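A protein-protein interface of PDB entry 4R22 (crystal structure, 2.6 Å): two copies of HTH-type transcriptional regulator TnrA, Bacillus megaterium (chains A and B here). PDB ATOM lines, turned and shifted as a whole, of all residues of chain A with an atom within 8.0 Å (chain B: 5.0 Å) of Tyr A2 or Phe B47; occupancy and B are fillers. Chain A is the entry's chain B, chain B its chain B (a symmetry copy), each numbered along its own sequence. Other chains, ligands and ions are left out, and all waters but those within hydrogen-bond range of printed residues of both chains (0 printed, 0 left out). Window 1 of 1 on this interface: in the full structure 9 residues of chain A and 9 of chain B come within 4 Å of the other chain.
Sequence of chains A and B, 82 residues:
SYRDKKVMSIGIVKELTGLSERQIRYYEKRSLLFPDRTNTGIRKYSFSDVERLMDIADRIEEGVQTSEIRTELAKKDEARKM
Tyr B2 touches its own counterpart, Tyr A2.
Tyr A2 touches Arg B3, and with the chains exchanged Arg A3 touches Tyr B2.
Tyr A2 touches Phe B47, and with the chains exchanged Phe A47 touches Tyr B2.
Lys A5 touches Phe B47, and with the chains exchanged Phe A47 touches Lys B5.
8 positions are printed for both chains.
Printed residues of chain B within 4 Å of Tyr A2: Tyr B2 (3.98 Å), Arg B3 (3.3 Å), Phe B47 (3.6 Å) and Glu B51 (2.4 Å).
Of chain A, only Tyr A2, Lys A5 and Val A7 come within 4 Å of Phe B47.
Of the printed residues of chain B, Val A7 touches Met B8 (3.5 Å) and Phe B47 (3.6 Å).
Printed residues of chain A within 4 Å of Glu B51: Tyr A2.
Of the printed residues of chain A, Met B8 touches Val A7 (3.5 Å).
Printed residues of chain B within 4 Å of Lys A5: Phe B47 (3.6 Å).
The nearest printed residue of chain B that does not touch Phe A47 is Phe B47 (4.2 Å).
OH of Tyr A2 lies within hydrogen-bond range of OE2 of Glu B51 (2.4 Å).
Among the printed residues, merely in contact across the chains: Arg A3 with Tyr B2 (3.3 Å), Tyr A2 with Arg B3 (3.3 Å), Val A7 with Met B8 (3.5 Å), Lys A5 with Phe B47 (3.6 Å), Phe A47 with Lys B5 (3.6 Å), Val A7 with Phe B47 (3.6 Å), Tyr A2 with Phe B47 (3.6 Å), Phe A47 with Tyr B2 (3.6 Å) and Tyr A2 with Tyr B2 (3.98 Å).
The backbone carbonyl oxygen of Arg A3 is in hydrogen-bond range of the backbone NH of Phe A47, 3.4 Å away.
The backbone NH (N) of Ser A48 sits at hydrogen-bond distance from the backbone carbonyl oxygen (O) of Arg A3 (2.6 Å).
N of Val A7 lies within hydrogen-bond range of O of Tyr A45 (2.8 Å).
N of Phe B47 is in hydrogen-bond range of O of Arg B3 (3.4 Å).
OE1 of Glu B51 lies within salt-bridge range of NH2 of Arg B3, at 2.8 Å.
The backbone carbonyl oxygen (O) of Met B8 lies within hydrogen-bond range of the backbone NH (N) of Tyr B45.
Of the 12 printed residues of chain A, 5 touch a printed residue of chain B.
Along chain A the printed residues that touch a printed residue of chain B span positions 2 to 47.
Among the printed residues, 10 pairs touch across the chains.
Among the printed residues, no Asp or Glu carboxylate lies within 4 Å of a Lys or Arg side-chain nitrogen of the other chain.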
ATOM      1  N   SER A   1      -3.818  32.832   5.886  1.00  0.00           N
ATOM      2  CA  SER A   1      -4.819  31.761   5.570  1.00  0.00           C
ATOM      3  C   SER A   1      -4.245  30.361   5.819  1.00  0.00           C
ATOM      4  O   SER A   1      -4.932  29.358   5.617  1.00  0.00           O
ATOM      5  CB  SER A   1      -5.242  31.861   4.107  1.00  0.00           C
ATOM      6  OG  SER A   1      -4.123  31.628   3.267  1.00  0.00           O
ATOM      7  N   TYR A   2      -2.983  30.311   6.238  1.00  0.00           N
ATOM      8  CA  TYR A   2      -2.285  29.064   6.524  1.00  0.00           C
ATOM      9  C   TYR A   2      -2.924  28.323   7.672  1.00  0.00           C
ATOM     10  O   TYR A   2      -2.932  27.099   7.712  1.00  0.00           O
ATOM     11  CB  TYR A   2      -0.846  29.358   6.921  1.00  0.00           C
ATOM     12  CG  TYR A   2      -0.070  30.116   5.887  1.00  0.00           C
ATOM     13  CD1 TYR A   2       0.857  31.090   6.262  1.00  0.00           C
ATOM     14  CD2 TYR A   2      -0.253  29.867   4.530  1.00  0.00           C
ATOM     15  CE1 TYR A   2       1.576  31.798   5.315  1.00  0.00           C
ATOM     16  CE2 TYR A   2       0.464  30.567   3.576  1.00  0.00           C
ATOM     17  CZ  TYR A   2       1.372  31.532   3.975  1.00  0.00           C
ATOM     18  OH  TYR A   2       2.068  32.239   3.033  1.00  0.00           O
ATOM     19  N   ARG A   3      -3.440  29.087   8.623  1.00  0.00           N
ATOM     20  CA  ARG A   3      -4.054  28.536   9.821  1.00  0.00           C
ATOM     21  C   ARG A   3      -5.116  27.470   9.631  1.00  0.00           C
ATOM     22  O   ARG A   3      -5.276  26.598  10.484  1.00  0.00           O
ATOM     23  CB  ARG A   3      -4.666  29.663  10.652  1.00  0.00           C
ATOM     24  CG  ARG A   3      -5.304  29.194  11.947  1.00  0.00           C
ATOM     25  CD  ARG A   3      -6.807  29.324  11.930  1.00  0.00           C
ATOM     26  NE  ARG A   3      -7.432  28.817  13.160  1.00  0.00           N
ATOM     27  CZ  ARG A   3      -7.071  29.189  14.381  1.00  0.00           C
ATOM     28  NH1 ARG A   3      -6.098  30.074  14.540  1.00  0.00           N
ATOM     29  NH2 ARG A   3      -7.656  28.654  15.437  1.00  0.00           N
ATOM     30  N   ASP A   4      -5.833  27.527   8.519  1.00  0.00           N
ATOM     31  CA  ASP A   4      -6.921  26.597   8.309  1.00  0.00           C
ATOM     32  C   ASP A   4      -6.741  25.593   7.186  1.00  0.00           C
ATOM     33  O   ASP A   4      -7.566  24.700   7.009  1.00  0.00           O
ATOM     34  CB  ASP A   4      -8.195  27.414   8.113  1.00  0.00           C
ATOM     35  CG  ASP A   4      -8.406  28.423   9.233  1.00  0.00           C
ATOM     36  OD1 ASP A   4      -8.725  27.996  10.364  1.00  0.00           O
ATOM     37  OD2 ASP A   4      -8.235  29.636   8.990  1.00  0.00           O
ATOM     38  N   LYS A   5      -5.661  25.750   6.430  1.00  0.00           N
ATOM     39  CA  LYS A   5      -5.334  24.863   5.322  1.00  0.00           C
ATOM     40  C   LYS A   5      -5.008  23.465   5.901  1.00  0.00           C
ATOM     41  O   LYS A   5      -4.145  23.347   6.779  1.00  0.00           O
ATOM     42  CB  LYS A   5      -4.122  25.445   4.577  1.00  0.00           C
ATOM     43  CG  LYS A   5      -4.012  25.077   3.095  1.00  0.00           C
ATOM     44  CD  LYS A   5      -5.113  25.734   2.268  1.00  0.00           C
ATOM     45  CE  LYS A   5      -5.096  25.268   0.816  1.00  0.00           C
ATOM     46  NZ  LYS A   5      -6.113  25.969  -0.042  1.00  0.00           N
ATOM     47  N   LYS A   6      -5.719  22.430   5.433  1.00  0.00           N
ATOM     48  CA  LYS A   6      -5.519  21.034   5.881  1.00  0.00           C
ATOM     49  C   LYS A   6      -4.296  20.485   5.156  1.00  0.00           C
ATOM     50  O   LYS A   6      -4.341  20.233   3.954  1.00  0.00           O
ATOM     51  CB  LYS A   6      -6.699  20.132   5.497  1.00  0.00           C
ATOM     52  CG  LYS A   6      -8.101  20.651   5.801  1.00  0.00           C
ATOM     53  CD  LYS A   6      -8.471  20.559   7.283  1.00  0.00           C
ATOM     54  CE  LYS A   6      -9.963  20.809   7.493  1.00  0.00           C
ATOM     55  NZ  LYS A   6     -10.316  20.896   8.933  1.00  0.00           N
ATOM     56  N   VAL A   7      -3.207  20.260   5.866  1.00  0.00           N
ATOM     57  CA  VAL A   7      -2.037  19.789   5.160  1.00  0.00           C
ATOM     58  C   VAL A   7      -1.204  18.766   5.902  1.00  0.00           C
ATOM     59  O   VAL A   7      -0.392  18.128   5.326  1.00  0.00           O
ATOM     60  CB  VAL A   7      -1.151  20.984   4.786  1.00  0.00           C
ATOM     61  CG1 VAL A   7      -1.716  21.697   3.564  1.00  0.00           C
ATOM     62  CG2 VAL A   7      -1.078  21.941   5.957  1.00  0.00           C
ATOM     63  N   MET A   8      -1.426  18.588   7.189  1.00  0.00           N
ATOM     64  CA  MET A   8      -0.606  17.654   7.932  1.00  0.00           C
ATOM     65  C   MET A   8      -1.268  16.369   8.417  1.00  0.00           C
ATOM     66  O   MET A   8      -2.285  16.401   9.100  1.00  0.00           O
ATOM     67  CB  MET A   8       0.055  18.391   9.100  1.00  0.00           C
ATOM     68  CG  MET A   8      -0.906  19.004  10.062  1.00  0.00           C
ATOM     69  SD  MET A   8      -0.082  20.222  11.116  1.00  0.00           S
ATOM     70  CE  MET A   8      -0.323  21.697  10.128  1.00  0.00           C
ATOM     71  N   TYR A  45      -4.932  17.340   8.488  1.00  0.00           N
ATOM     72  CA  TYR A  45      -5.365  18.336   9.451  1.00  0.00           C
ATOM     73  C   TYR A  45      -4.727  19.692   9.191  1.00  0.00           C
ATOM     74  O   TYR A  45      -3.674  19.786   8.566  1.00  0.00           O
ATOM     75  CB  TYR A  45      -5.033  17.902  10.869  1.00  0.00           C
ATOM     76  CG  TYR A  45      -5.491  16.519  11.206  1.00  0.00           C
ATOM     77  CD1 TYR A  45      -4.803  15.411  10.735  1.00  0.00           C
ATOM     78  CD2 TYR A  45      -6.595  16.311  12.027  1.00  0.00           C
ATOM     79  CE1 TYR A  45      -5.193  14.121  11.078  1.00  0.00           C
ATOM     80  CE2 TYR A  45      -6.991  15.031  12.373  1.00  0.00           C
ATOM     81  CZ  TYR A  45      -6.285  13.937  11.900  1.00  0.00           C
ATOM     82  OH  TYR A  45      -6.653  12.672  12.295  1.00  0.00           O
ATOM     83  N   SER A  46      -5.375  20.745   9.684  1.00  0.00           N
ATOM     84  CA  SER A  46      -4.861  22.102   9.534  1.00  0.00           C
ATOM     85  C   SER A  46      -4.457  22.600  10.913  1.00  0.00           C
ATOM     86  O   SER A  46      -4.849  22.010  11.928  1.00  0.00           O
ATOM     87  CB  SER A  46      -5.933  23.028   8.978  1.00  0.00           C
ATOM     88  OG  SER A  46      -6.824  23.423  10.006  1.00  0.00           O
ATOM     89  N   PHE A  47      -3.684  23.686  10.946  1.00  0.00           N
ATOM     90  CA  PHE A  47      -3.218  24.274  12.210  1.00  0.00           C
ATOM     91  C   PHE A  47      -4.381  24.627  13.102  1.00  0.00           C
ATOM     92  O   PHE A  47      -4.269  24.632  14.334  1.00  0.00           O
ATOM     93  CB  PHE A  47      -2.388  25.533  11.966  1.00  0.00           C
ATOM     94  CG  PHE A  47      -0.964  25.257  11.681  1.00  0.00           C
ATOM     95  CD1 PHE A  47      -0.439  25.498  10.420  1.00  0.00           C
ATOM     96  CD2 PHE A  47      -0.152  24.694  12.654  1.00  0.00           C
ATOM     97  CE1 PHE A  47       0.886  25.188  10.129  1.00  0.00           C
ATOM     98  CE2 PHE A  47       1.176  24.377  12.376  1.00  0.00           C
ATOM     99  CZ  PHE A  47       1.695  24.621  11.108  1.00  0.00           C
ATOM    100  N   SER A  48      -5.498  24.949  12.471  1.00  0.00           N
ATOM    101  CA  SER A  48      -6.688  25.280  13.214  1.00  0.00           C
ATOM    102  C   SER A  48      -7.187  24.032  13.943  1.00  0.00           C
ATOM    103  O   SER A  48      -7.588  24.118  15.111  1.00  0.00           O
ATOM    104  CB  SER A  48      -7.746  25.815  12.272  1.00  0.00           C
ATOM    105  OG  SER A  48      -9.016  25.633  12.841  1.00  0.00           O
ATOM    106  N   TYR B   2       2.599  30.179  11.599  1.00  0.00           N
ATOM    107  CA  TYR B   2       2.252  28.956  10.885  1.00  0.00           C
ATOM    108  C   TYR B   2       3.015  28.839   9.587  1.00  0.00           C
ATOM    109  O   TYR B   2       3.353  27.747   9.147  1.00  0.00           O
ATOM    110  CB  TYR B   2       0.771  28.962  10.539  1.00  0.00           C
ATOM    111  CG  TYR B   2      -0.132  29.095  11.728  1.00  0.00           C
ATOM    112  CD1 TYR B   2      -1.306  29.847  11.652  1.00  0.00           C
ATOM    113  CD2 TYR B   2       0.175  28.472  12.934  1.00  0.00           C
ATOM    114  CE1 TYR B   2      -2.145  29.979  12.745  1.00  0.00           C
ATOM    115  CE2 TYR B   2      -0.659  28.595  14.031  1.00  0.00           C
ATOM    116  CZ  TYR B   2      -1.813  29.352  13.929  1.00  0.00           C
ATOM    117  OH  TYR B   2      -2.630  29.491  15.018  1.00  0.00           O
ATOM    118  N   ARG B   3       3.258  29.984   8.968  1.00  0.00           N
ATOM    119  CA  ARG B   3       3.942  30.047   7.685  1.00  0.00           C
ATOM    120  C   ARG B   3       5.261  29.310   7.562  1.00  0.00           C
ATOM    121  O   ARG B   3       5.612  28.847   6.478  1.00  0.00           O
ATOM    122  CB  ARG B   3       4.184  31.507   7.303  1.00  0.00           C
ATOM    123  CG  ARG B   3       4.864  31.684   5.957  1.00  0.00           C
ATOM    124  CD  ARG B   3       6.274  32.204   6.086  1.00  0.00           C
ATOM    125  NE  ARG B   3       6.954  32.322   4.790  1.00  0.00           N
ATOM    126  CZ  ARG B   3       6.449  32.963   3.744  1.00  0.00           C
ATOM    127  NH1 ARG B   3       5.266  33.551   3.839  1.00  0.00           N
ATOM    128  NH2 ARG B   3       7.107  32.987   2.599  1.00  0.00           N
ATOM    129  N   LYS B   5       6.403  26.847  10.038  1.00  0.00           N
ATOM    130  CA  LYS B   5       6.382  25.590  10.776  1.00  0.00           C
ATOM    131  C   LYS B   5       6.421  24.430   9.753  1.00  0.00           C
ATOM    132  O   LYS B   5       5.583  24.378   8.846  1.00  0.00           O
ATOM    133  CB  LYS B   5       5.094  25.541  11.613  1.00  0.00           C
ATOM    134  CG  LYS B   5       5.158  24.690  12.884  1.00  0.00           C
ATOM    135  CD  LYS B   5       6.077  25.310  13.932  1.00  0.00           C
ATOM    136  CE  LYS B   5       6.255  24.405  15.146  1.00  0.00           C
ATOM    137  NZ  LYS B   5       7.083  25.033  16.234  1.00  0.00           N
ATOM    138  N   MET B   8       4.244  19.472   6.760  1.00  0.00           N
ATOM    139  CA  MET B   8       3.674  18.649   5.713  1.00  0.00           C
ATOM    140  C   MET B   8       4.637  17.827   4.863  1.00  0.00           C
ATOM    141  O   MET B   8       5.573  18.359   4.278  1.00  0.00           O
ATOM    142  CB  MET B   8       2.783  19.521   4.824  1.00  0.00           C
ATOM    143  CG  MET B   8       3.495  20.654   4.165  1.00  0.00           C
ATOM    144  SD  MET B   8       2.322  21.879   3.534  1.00  0.00           S
ATOM    145  CE  MET B   8       2.199  22.952   4.964  1.00  0.00           C
ATOM    146  N   LEU B  16       0.191  20.899  -3.599  1.00  0.00           N
ATOM    147  CA  LEU B  16       0.147  22.352  -3.465  1.00  0.00           C
ATOM    148  C   LEU B  16       0.976  23.073  -4.512  1.00  0.00           C
ATOM    149  O   LEU B  16       0.648  24.184  -4.903  1.00  0.00           O
ATOM    150  CB  LEU B  16       0.646  22.775  -2.078  1.00  0.00           C
ATOM    151  CG  LEU B  16      -0.391  23.158  -1.016  1.00  0.00           C
ATOM    152  CD1 LEU B  16      -1.399  22.059  -0.877  1.00  0.00           C
ATOM    153  CD2 LEU B  16       0.280  23.421   0.328  1.00  0.00           C
ATOM    154  N   TYR B  45       7.892  19.725   5.289  1.00  0.00           N
ATOM    155  CA  TYR B  45       7.992  21.061   4.731  1.00  0.00           C
ATOM    156  C   TYR B  45       7.022  22.028   5.393  1.00  0.00           C
ATOM    157  O   TYR B  45       6.014  21.620   5.964  1.00  0.00           O
ATOM    158  CB  TYR B  45       7.724  21.046   3.234  1.00  0.00           C
ATOM    159  CG  TYR B  45       8.524  20.032   2.482  1.00  0.00           C
ATOM    160  CD1 TYR B  45       8.186  18.688   2.528  1.00  0.00           C
ATOM    161  CD2 TYR B  45       9.603  20.414   1.692  1.00  0.00           C
ATOM    162  CE1 TYR B  45       8.896  17.741   1.798  1.00  0.00           C
ATOM    163  CE2 TYR B  45      10.315  19.479   0.961  1.00  0.00           C
ATOM    164  CZ  TYR B  45       9.956  18.142   1.013  1.00  0.00           C
ATOM    165  OH  TYR B  45      10.636  17.229   0.241  1.00  0.00           O
ATOM    166  N   SER B  46       7.335  23.319   5.306  1.00  0.00           N
ATOM    167  CA  SER B  46       6.479  24.356   5.871  1.00  0.00           C
ATOM    168  C   SER B  46       5.891  25.151   4.716  1.00  0.00           C
ATOM    169  O   SER B  46       6.380  25.059   3.583  1.00  0.00           O
ATOM    170  CB  SER B  46       7.284  25.300   6.751  1.00  0.00           C
ATOM    171  OG  SER B  46       7.985  26.240   5.954  1.00  0.00           O
ATOM    172  N   PHE B  47       4.851  25.934   5.007  1.00  0.00           N
ATOM    173  CA  PHE B  47       4.184  26.755   3.987  1.00  0.00           C
ATOM    174  C   PHE B  47       5.164  27.686   3.317  1.00  0.00           C
ATOM    175  O   PHE B  47       4.997  28.066   2.152  1.00  0.00           O
ATOM    176  CB  PHE B  47       3.056  27.588   4.594  1.00  0.00           C
ATOM    177  CG  PHE B  47       1.775  26.857   4.704  1.00  0.00           C
ATOM    178  CD1 PHE B  47       1.265  26.516   5.948  1.00  0.00           C
ATOM    179  CD2 PHE B  47       1.102  26.448   3.563  1.00  0.00           C
ATOM    180  CE1 PHE B  47       0.089  25.780   6.057  1.00  0.00           C
ATOM    181  CE2 PHE B  47      -0.076  25.709   3.658  1.00  0.00           C
ATOM    182  CZ  PHE B  47      -0.581  25.370   4.909  1.00  0.00           C
ATOM    183  N   SER B  48       6.180  28.072   4.072  1.00  0.00           N
ATOM    184  CA  SER B  48       7.198  28.940   3.536  1.00  0.00           C
ATOM    185  C   SER B  48       7.983  28.188   2.460  1.00  0.00           C
ATOM    186  O   SER B  48       8.290  28.759   1.407  1.00  0.00           O
ATOM    187  CB  SER B  48       8.114  29.400   4.650  1.00  0.00           C
ATOM    188  OG  SER B  48       9.358  29.769   4.114  1.00  0.00           O
ATOM    189  N   ASP B  49       8.295  26.907   2.711  1.00  0.00           N
ATOM    190  CA  ASP B  49       9.027  26.089   1.730  1.00  0.00           C
ATOM    191  C   ASP B  49       8.143  25.924   0.484  1.00  0.00           C
ATOM    192  O   ASP B  49       8.646  25.948  -0.643  1.00  0.00           O
ATOM    193  CB  ASP B  49       9.393  24.688   2.279  1.00  0.00           C
ATOM    194  CG  ASP B  49      10.401  24.724   3.452  1.00  0.00           C
ATOM    195  OD1 ASP B  49      11.452  25.405   3.359  1.00  0.00           O
ATOM    196  OD2 ASP B  49      10.143  24.035   4.469  1.00  0.00           O
ATOM    197  N   VAL B  50       6.834  25.760   0.682  1.00  0.00           N
ATOM    198  CA  VAL B  50       5.899  25.615  -0.439  1.00  0.00           C
ATOM    199  C   VAL B  50       6.033  26.789  -1.421  1.00  0.00           C
ATOM    200  O   VAL B  50       6.097  26.586  -2.640  1.00  0.00           O
ATOM    201  CB  VAL B  50       4.422  25.517   0.062  1.00  0.00           C
ATOM    202  CG1 VAL B  50       3.447  25.573  -1.104  1.00  0.00           C
ATOM    203  CG2 VAL B  50       4.224  24.228   0.834  1.00  0.00           C
ATOM    204  N   GLU B  51       6.082  28.012  -0.892  1.00  0.00           N
ATOM    205  CA  GLU B  51       6.227  29.213  -1.727  1.00  0.00           C
ATOM    206  C   GLU B  51       7.619  29.252  -2.358  1.00  0.00           C
ATOM    207  O   GLU B  51       7.772  29.556  -3.543  1.00  0.00           O
ATOM    208  CB  GLU B  51       6.014  30.464  -0.879  1.00  0.00           C
ATOM    209  CG  GLU B  51       4.690  30.504  -0.157  1.00  0.00           C
ATOM    210  CD  GLU B  51       4.654  31.596   0.886  1.00  0.00           C
ATOM    211  OE1 GLU B  51       5.185  32.691   0.605  1.00  0.00           O
ATOM    212  OE2 GLU B  51       4.092  31.365   1.978  1.00  0.00           O
